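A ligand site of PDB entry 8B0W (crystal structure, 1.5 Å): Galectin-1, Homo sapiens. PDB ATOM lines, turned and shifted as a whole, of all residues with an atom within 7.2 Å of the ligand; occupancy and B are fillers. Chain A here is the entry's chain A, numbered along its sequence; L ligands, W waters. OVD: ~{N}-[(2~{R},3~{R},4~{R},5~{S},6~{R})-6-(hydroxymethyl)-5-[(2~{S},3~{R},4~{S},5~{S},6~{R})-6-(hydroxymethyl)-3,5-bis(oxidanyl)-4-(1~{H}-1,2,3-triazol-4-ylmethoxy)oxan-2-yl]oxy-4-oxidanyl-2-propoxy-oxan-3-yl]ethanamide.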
ATOM      1  N   VAL A  30      13.451  31.117 -17.655  1.00  0.00           N
ATOM      2  CA  VAL A  30      13.030  30.179 -18.672  1.00  0.00           C
ATOM      3  C   VAL A  30      14.188  29.260 -19.025  1.00  0.00           C
ATOM      4  O   VAL A  30      15.329  29.726 -19.228  1.00  0.00           O
ATOM      5  CB  VAL A  30      12.546  30.912 -19.928  1.00  0.00           C
ATOM      6  CG1 VAL A  30      12.336  29.917 -21.084  1.00  0.00           C
ATOM      7  CG2 VAL A  30      11.276  31.672 -19.660  1.00  0.00           C
ATOM      8  N   ASN A  32      14.355  26.567 -22.145  1.00  0.00           N
ATOM      9  CA  ASN A  32      13.719  25.995 -23.324  1.00  0.00           C
ATOM     10  C   ASN A  32      14.569  24.862 -23.862  1.00  0.00           C
ATOM     11  O   ASN A  32      15.782  25.027 -24.029  1.00  0.00           O
ATOM     12  CB  ASN A  32      13.546  27.042 -24.411  1.00  0.00           C
ATOM     13  CG  ASN A  32      12.472  28.027 -24.126  1.00  0.00           C
ATOM     14  OD1 ASN A  32      11.515  27.754 -23.371  1.00  0.00           O
ATOM     15  ND2 ASN A  32      12.599  29.196 -24.719  1.00  0.00           N
ATOM     16  N   HIS A  43       9.214  24.102 -22.559  1.00  0.00           N
ATOM     17  CA  HIS A  43       9.367  25.477 -22.119  1.00  0.00           C
ATOM     18  C   HIS A  43       9.093  25.438 -20.633  1.00  0.00           C
ATOM     19  O   HIS A  43       7.959  25.144 -20.223  1.00  0.00           O
ATOM     20  CB  HIS A  43       8.380  26.379 -22.818  1.00  0.00           C
ATOM     21  CG  HIS A  43       8.244  27.751 -22.261  1.00  0.00           C
ATOM     22  ND1 HIS A  43       9.179  28.745 -22.473  1.00  0.00           N
ATOM     23  CD2 HIS A  43       7.252  28.323 -21.535  1.00  0.00           C
ATOM     24  CE1 HIS A  43       8.768  29.864 -21.896  1.00  0.00           C
ATOM     25  NE2 HIS A  43       7.587  29.627 -21.341  1.00  0.00           N
ATOM     26  N   ASN A  45       9.196  27.409 -17.152  1.00  0.00           N
ATOM     27  CA  ASN A  45       9.120  28.820 -16.790  1.00  0.00           C
ATOM     28  C   ASN A  45       8.661  29.008 -15.346  1.00  0.00           C
ATOM     29  O   ASN A  45       7.483  29.269 -15.077  1.00  0.00           O
ATOM     30  CB  ASN A  45       8.225  29.551 -17.798  1.00  0.00           C
ATOM     31  CG  ASN A  45       8.043  31.020 -17.521  1.00  0.00           C
ATOM     32  OD1 ASN A  45       7.039  31.588 -17.925  1.00  0.00           O
ATOM     33  ND2 ASN A  45       9.000  31.640 -16.886  1.00  0.00           N
ATOM     34  N   ARG A  47       7.783  31.182 -12.485  1.00  0.00           N
ATOM     35  CA  ARG A  47       7.354  32.573 -12.338  1.00  0.00           C
ATOM     36  C   ARG A  47       7.325  32.931 -10.852  1.00  0.00           C
ATOM     37  O   ARG A  47       6.519  32.386 -10.097  1.00  0.00           O
ATOM     38  CB  ARG A  47       6.001  32.802 -13.012  1.00  0.00           C
ATOM     39  CG  ARG A  47       6.077  32.619 -14.492  1.00  0.00           C
ATOM     40  CD  ARG A  47       4.715  32.775 -15.157  1.00  0.00           C
ATOM     41  NE  ARG A  47       4.799  32.510 -16.586  1.00  0.00           N
ATOM     42  CZ  ARG A  47       3.783  32.595 -17.437  1.00  0.00           C
ATOM     43  NH1 ARG A  47       2.579  32.968 -17.033  1.00  0.00           N
ATOM     44  NH2 ARG A  47       3.986  32.285 -18.714  1.00  0.00           N
ATOM     45  N   ALA A  50       5.338  37.195 -12.210  1.00  0.00           N
ATOM     46  CA  ALA A  50       5.300  37.506 -13.638  1.00  0.00           C
ATOM     47  C   ALA A  50       3.974  37.035 -14.207  1.00  0.00           C
ATOM     48  O   ALA A  50       3.465  35.973 -13.838  1.00  0.00           O
ATOM     49  CB  ALA A  50       6.443  36.833 -14.395  1.00  0.00           C
ATOM     50  N   HIS A  51       3.428  37.823 -15.138  1.00  0.00           N
ATOM     51  CA  HIS A  51       2.169  37.500 -15.822  1.00  0.00           C
ATOM     52  C   HIS A  51       1.029  37.286 -14.828  1.00  0.00           C
ATOM     53  O   HIS A  51       0.127  36.470 -15.053  1.00  0.00           O
ATOM     54  CB  HIS A  51       2.326  36.278 -16.718  1.00  0.00           C
ATOM     55  CG  HIS A  51       3.297  36.479 -17.843  1.00  0.00           C
ATOM     56  ND1 HIS A  51       4.650  36.291 -17.703  1.00  0.00           N
ATOM     57  CD2 HIS A  51       3.091  36.844 -19.134  1.00  0.00           C
ATOM     58  CE1 HIS A  51       5.249  36.532 -18.854  1.00  0.00           C
ATOM     59  NE2 HIS A  51       4.330  36.877 -19.738  1.00  0.00           N
ATOM     60  N   ASP A  53       1.251  35.872 -12.053  1.00  0.00           N
ATOM     61  CA  ASP A  53       1.466  34.620 -11.358  1.00  0.00           C
ATOM     62  C   ASP A  53       2.544  34.800 -10.300  1.00  0.00           C
ATOM     63  O   ASP A  53       3.528  35.511 -10.527  1.00  0.00           O
ATOM     64  CB  ASP A  53       1.891  33.516 -12.337  1.00  0.00           C
ATOM     65  CG  ASP A  53       0.819  33.193 -13.341  1.00  0.00           C
ATOM     66  OD1 ASP A  53       1.150  32.857 -14.494  1.00  0.00           O
ATOM     67  OD2 ASP A  53      -0.386  33.248 -12.979  1.00  0.00           O
ATOM     68  N   VAL A  58       5.239  27.310 -14.741  1.00  0.00           N
ATOM     69  CA  VAL A  58       4.466  27.210 -15.963  1.00  0.00           C
ATOM     70  C   VAL A  58       5.281  26.403 -16.960  1.00  0.00           C
ATOM     71  O   VAL A  58       6.447  26.707 -17.231  1.00  0.00           O
ATOM     72  CB  VAL A  58       4.156  28.602 -16.526  1.00  0.00           C
ATOM     73  CG1 VAL A  58       3.516  28.500 -17.906  1.00  0.00           C
ATOM     74  CG2 VAL A  58       3.264  29.378 -15.569  1.00  0.00           C
ATOM     75  N   CYS A  59       4.680  25.383 -17.552  1.00  0.00           N
ATOM     76  CA  CYS A  59       5.314  24.629 -18.638  1.00  0.00           C
ATOM     77  C   CYS A  59       4.451  24.642 -19.888  1.00  0.00           C
ATOM     78  O   CYS A  59       3.214  24.706 -19.800  1.00  0.00           O
ATOM     79  CB  CYS A  59       5.556  23.187 -18.289  1.00  0.00           C
ATOM     80  SG  CYS A  59       6.686  22.962 -16.889  1.00  0.00           S
ATOM     81  N   ASN A  60       5.101  24.541 -21.040  1.00  0.00           N
ATOM     82  CA  ASN A  60       4.390  24.425 -22.303  1.00  0.00           C
ATOM     83  C   ASN A  60       5.318  23.791 -23.318  1.00  0.00           C
ATOM     84  O   ASN A  60       6.497  23.550 -23.058  1.00  0.00           O
ATOM     85  CB  ASN A  60       3.880  25.795 -22.777  1.00  0.00           C
ATOM     86  CG  ASN A  60       2.606  25.672 -23.602  1.00  0.00           C
ATOM     87  OD1 ASN A  60       2.284  24.588 -24.084  1.00  0.00           O
ATOM     88  ND2 ASN A  60       1.952  26.790 -23.831  1.00  0.00           N
ATOM     89  N   SER A  61       4.770  23.504 -24.490  1.00  0.00           N
ATOM     90  CA  SER A  61       5.508  23.094 -25.676  1.00  0.00           C
ATOM     91  C   SER A  61       5.305  24.147 -26.753  1.00  0.00           C
ATOM     92  O   SER A  61       4.453  25.039 -26.647  1.00  0.00           O
ATOM     93  CB  SER A  61       5.006  21.726 -26.175  1.00  0.00           C
ATOM     94  OG  SER A  61       3.600  21.791 -26.430  1.00  0.00           O
ATOM     95  N   LYS A  62       6.139  24.059 -27.791  1.00  0.00           N
ATOM     96  CA  LYS A  62       5.997  24.900 -28.970  1.00  0.00           C
ATOM     97  C   LYS A  62       6.267  23.997 -30.171  1.00  0.00           C
ATOM     98  O   LYS A  62       7.300  23.330 -30.245  1.00  0.00           O
ATOM     99  CB  LYS A  62       6.910  26.120 -28.924  1.00  0.00           C
ATOM    100  CG  LYS A  62       6.578  27.132 -30.042  1.00  0.00           C
ATOM    101  CD  LYS A  62       7.548  28.302 -30.113  1.00  0.00           C
ATOM    102  CE  LYS A  62       7.010  29.526 -29.384  1.00  0.00           C
ATOM    103  NZ  LYS A  62       8.029  30.625 -29.380  1.00  0.00           N
ATOM    104  N   TRP A  67       2.495  27.790 -29.724  1.00  0.00           N
ATOM    105  CA  TRP A  67       2.423  27.359 -28.336  1.00  0.00           C
ATOM    106  C   TRP A  67       1.350  26.291 -28.165  1.00  0.00           C
ATOM    107  O   TRP A  67       0.243  26.390 -28.723  1.00  0.00           O
ATOM    108  CB  TRP A  67       2.099  28.540 -27.435  1.00  0.00           C
ATOM    109  CG  TRP A  67       3.194  29.493 -27.226  1.00  0.00           C
ATOM    110  CD1 TRP A  67       3.215  30.803 -27.607  1.00  0.00           C
ATOM    111  CD2 TRP A  67       4.426  29.244 -26.535  1.00  0.00           C
ATOM    112  NE1 TRP A  67       4.384  31.378 -27.213  1.00  0.00           N
ATOM    113  CE2 TRP A  67       5.146  30.450 -26.545  1.00  0.00           C
ATOM    114  CE3 TRP A  67       4.978  28.125 -25.908  1.00  0.00           C
ATOM    115  CZ2 TRP A  67       6.418  30.571 -25.970  1.00  0.00           C
ATOM    116  CZ3 TRP A  67       6.241  28.245 -25.329  1.00  0.00           C
ATOM    117  CH2 TRP A  67       6.939  29.453 -25.365  1.00  0.00           C
ATOM    118  N   GLY A  68       1.674  25.261 -27.377  1.00  0.00           N
ATOM    119  CA  GLY A  68       0.703  24.272 -26.979  1.00  0.00           C
ATOM    120  C   GLY A  68      -0.140  24.713 -25.805  1.00  0.00           C
ATOM    121  O   GLY A  68      -0.268  25.892 -25.477  1.00  0.00           O
ATOM    122  N   THR A  69      -0.754  23.704 -25.193  1.00  0.00           N
ATOM    123  CA  THR A  69      -1.589  23.899 -24.018  1.00  0.00           C
ATOM    124  C   THR A  69      -0.713  23.994 -22.756  1.00  0.00           C
ATOM    125  O   THR A  69      -0.033  23.029 -22.387  1.00  0.00           O
ATOM    126  CB  THR A  69      -2.615  22.766 -23.913  1.00  0.00           C
ATOM    127  OG1 THR A  69      -3.433  22.695 -25.103  1.00  0.00           O
ATOM    128  CG2 THR A  69      -3.504  23.010 -22.751  1.00  0.00           C
ATOM    129  N   GLU A  70      -0.734  25.146 -22.110  1.00  0.00           N
ATOM    130  CA  GLU A  70       0.007  25.376 -20.876  1.00  0.00           C
ATOM    131  C   GLU A  70      -0.467  24.496 -19.735  1.00  0.00           C
ATOM    132  O   GLU A  70      -1.651  24.171 -19.626  1.00  0.00           O
ATOM    133  CB  GLU A  70      -0.162  26.848 -20.483  1.00  0.00           C
ATOM    134  CG  GLU A  70       0.813  27.416 -19.569  1.00  0.00           C
ATOM    135  CD  GLU A  70       0.471  28.844 -19.245  1.00  0.00           C
ATOM    136  OE1 GLU A  70       0.625  29.692 -20.163  1.00  0.00           O
ATOM    137  OE2 GLU A  70       0.079  29.126 -18.100  1.00  0.00           O
ATOM    138  N   GLN A  71       0.474  24.085 -18.897  1.00  0.00           N
ATOM    139  CA  GLN A  71       0.214  23.355 -17.663  1.00  0.00           C
ATOM    140  C   GLN A  71       0.977  24.023 -16.543  1.00  0.00           C
ATOM    141  O   GLN A  71       2.098  24.518 -16.735  1.00  0.00           O
ATOM    142  CB  GLN A  71       0.663  21.901 -17.780  1.00  0.00           C
ATOM    143  CG  GLN A  71      -0.085  21.188 -18.873  1.00  0.00           C
ATOM    144  CD  GLN A  71       0.155  19.717 -18.866  1.00  0.00           C
ATOM    145  OE1 GLN A  71       1.067  19.228 -18.207  1.00  0.00           O
ATOM    146  NE2 GLN A  71      -0.688  18.987 -19.603  1.00  0.00           N
ATOM    147  N   ARG A  72       0.442  23.969 -15.340  1.00  0.00           N
ATOM    148  CA  ARG A  72       1.111  24.494 -14.173  1.00  0.00           C
ATOM    149  C   ARG A  72       1.326  23.416 -13.127  1.00  0.00           C
ATOM    150  O   ARG A  72       0.545  22.467 -13.003  1.00  0.00           O
ATOM    151  CB  ARG A  72       0.307  25.659 -13.616  1.00  0.00           C
ATOM    152  CG  ARG A  72       0.295  26.818 -14.592  1.00  0.00           C
ATOM    153  CD  ARG A  72      -0.689  27.894 -14.297  1.00  0.00           C
ATOM    154  NE  ARG A  72      -0.493  28.969 -15.264  1.00  0.00           N
ATOM    155  CZ  ARG A  72      -0.498  30.257 -14.975  1.00  0.00           C
ATOM    156  NH1 ARG A  72      -0.781  30.696 -13.754  1.00  0.00           N
ATOM    157  NH2 ARG A  72      -0.201  31.124 -15.938  1.00  0.00           N
ATOM    158  N   ASP A 122      16.813  32.031 -20.430  1.00  0.00           N
ATOM    159  CA  ASP A 122      16.468  33.424 -20.478  1.00  0.00           C
ATOM    160  C   ASP A 122      16.029  33.834 -19.085  1.00  0.00           C
ATOM    161  O   ASP A 122      15.652  32.990 -18.261  1.00  0.00           O
ATOM    162  CB  ASP A 122      15.357  33.724 -21.477  1.00  0.00           C
ATOM    163  CG  ASP A 122      15.625  33.161 -22.858  1.00  0.00           C
ATOM    164  OD1 ASP A 122      16.792  33.117 -23.285  1.00  0.00           O
ATOM    165  OD2 ASP A 122      14.642  32.807 -23.537  1.00  0.00           O
ATOM    166  N   GLY A 123      16.076  35.127 -18.826  1.00  0.00           N
ATOM    167  CA  GLY A 123      15.509  35.629 -17.594  1.00  0.00           C
ATOM    168  C   GLY A 123      16.483  35.642 -16.435  1.00  0.00           C
ATOM    169  O   GLY A 123      17.706  35.672 -16.617  1.00  0.00           O
HETATM  170  C4  OVD L   1       0.711  33.517 -21.223  1.00  0.00           C
HETATM  171  C5  OVD L   1      -0.113  34.647 -21.797  1.00  0.00           C
HETATM  172  C6  OVD L   1       0.374  35.041 -23.185  1.00  0.00           C
HETATM  173  C7  OVD L   1      -2.584  31.673 -18.171  1.00  0.00           C
HETATM  174  C8  OVD L   1      -3.071  31.730 -16.674  1.00  0.00           C
HETATM  175  N2  OVD L   1      -1.826  32.714 -18.570  1.00  0.00           N
HETATM  176  C3  OVD L   1       0.174  33.257 -19.838  1.00  0.00           C
HETATM  177  C1  OVD L   1      -2.054  33.923 -20.681  1.00  0.00           C
HETATM  178  C2  OVD L   1      -1.299  32.841 -19.940  1.00  0.00           C
HETATM  179  CAF OVD L   1      -4.247  33.818 -19.831  1.00  0.00           C
HETATM  180  CAM OVD L   1      -5.506  34.281 -20.444  1.00  0.00           C
HETATM  181  CAO OVD L   1       3.871  29.687 -22.354  1.00  0.00           C
HETATM  182  CAP OVD L   1       4.246  33.913 -21.957  1.00  0.00           C
HETATM  183  CAQ OVD L   1       5.257  33.215 -22.835  1.00  0.00           C
HETATM  184  CAR OVD L   1       5.282  31.756 -22.413  1.00  0.00           C
HETATM  185  CAS OVD L   1       3.848  31.198 -22.539  1.00  0.00           C
HETATM  186  CAU OVD L   1       2.895  33.238 -22.020  1.00  0.00           C
HETATM  187  CAY OVD L   1      -6.802  34.164 -19.734  1.00  0.00           C
HETATM  188  CAZ OVD L   1       7.400  33.134 -23.457  1.00  0.00           C
HETATM  189  CBA OVD L   1       8.677  34.029 -23.301  1.00  0.00           C
HETATM  190  CBB OVD L   1       8.757  35.309 -23.620  1.00  0.00           C
HETATM  191  NBC OVD L   1      10.001  35.659 -23.297  1.00  0.00           N
HETATM  192  NBD OVD L   1      10.599  34.646 -22.822  1.00  0.00           N
HETATM  193  NBE OVD L   1       9.850  33.666 -22.790  1.00  0.00           N
HETATM  194  O1  OVD L   1      -3.388  33.481 -20.959  1.00  0.00           O
HETATM  195  O3  OVD L   1       0.880  32.209 -19.208  1.00  0.00           O
HETATM  196  O4  OVD L   1       2.060  33.940 -21.131  1.00  0.00           O
HETATM  197  O5  OVD L   1      -1.467  34.211 -21.960  1.00  0.00           O
HETATM  198  O6  OVD L   1       0.205  33.929 -24.054  1.00  0.00           O
HETATM  199  O7  OVD L   1      -2.900  30.740 -18.920  1.00  0.00           O
HETATM  200  OAN OVD L   1       4.114  35.270 -22.381  1.00  0.00           O
HETATM  201  OAT OVD L   1       2.991  31.845 -21.585  1.00  0.00           O
HETATM  202  OAV OVD L   1       5.811  31.682 -21.037  1.00  0.00           O
HETATM  203  OAW OVD L   1       2.534  29.187 -22.192  1.00  0.00           O
HETATM  204  OAX OVD L   1       6.502  33.841 -22.645  1.00  0.00           O
HETATM  205  O   HOH W   1      10.446  31.298 -24.453  1.00  0.00           O
HETATM  206  O   HOH W   2       7.434  33.908 -19.660  1.00  0.00           O
HETATM  207  O   HOH W   3      -0.825  34.310 -16.354  1.00  0.00           O
HETATM  208  O   HOH W   4      -6.015  30.400 -19.435  1.00  0.00           O
HETATM  209  O   HOH W   5       0.336  30.251 -24.213  1.00  0.00           O
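ND2 of Asn 60 lies within hydrogen-bond range of O of Gly 68 (2.9 Å).
The backbone NH of Asn 45 is in hydrogen-bond range of the backbone carbonyl oxygen of Val 58 (2.8 Å).
N of His 43 lies within hydrogen-bond range of O of Asn 60 (2.8 Å).
OD1 of Asp 53 lies within salt-bridge range of NH2 of Arg 72, at 2.6 Å.
The guanidinium group (NE) of Arg 47 sits at hydrogen-bond distance from the side-chain amide oxygen (OD1) of Asn 45, at 2.8 Å.
O of Thr 69 sits close to OD1 of Asn 60, at 3.3 Å.
The side-chain carboxylate (OD1) of Asp 53 is in salt-bridge range of the guanidinium group (NH1) of Arg 47, at 2.9 Å.
ND1 of His 43 is in hydrogen-bond range of OD1 of Asn 32 (2.7 Å).
N2 of the ligand sits close to NH2 of Arg 72 (3.5 Å).
CG2 of Val 30 touches NBE of the ligand, 3.98 Å away.
Trp 67 touches the ligand (CZ2 to CAZ, 3.7 Å).
Hydrophobic or aromatic side chains that line the ligand: Val 30, His 43, His 51 and Trp 67.
The nearest printed residue that does not touch the ligand is Val 58 (4.5 Å).
Water W3 lies within hydrogen-bond range of the backbone carbonyl oxygen (O) of His 51 (2.7 Å), a nitrogen (N2) of the ligand (2.9 Å), the side-chain carboxylate (OD1) of Asp 53 (3.1 Å) and the guanidinium group (NH2) of Arg 72 (3.3 Å).
Water W1 lies within hydrogen-bond range of a nitrogen (NBE) of the ligand, the side-chain amide nitrogen (ND2) of Asn 32 and a ring nitrogen (ND1) of His 43.
Water W2 bridges OD1 of Asn 45 (2.9 Å) and OAV of the ligand (3.1 Å).
The side-chain amide oxygen (OD1) of Asn 45 lies within hydrogen-bond range of an oxygen (OAV) of the ligand (3.3 Å).
NH1 of Arg 47 lies within hydrogen-bond range of O3 of the ligand (2.9 Å).
The side-chain amide nitrogen (ND2) of Asn 60 is in hydrogen-bond range of an oxygen (OAW) of the ligand.
An oxygen (O3) of the ligand is in hydrogen-bond range of the side-chain carboxylate of Glu 70 (2.7 Å).
An oxygen (OAN) of the ligand sits at hydrogen-bond distance from a ring nitrogen (NE2) of His 51 (3.1 Å).
OAV of the ligand sits at hydrogen-bond distance from NE2 of His 43 (2.7 Å).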
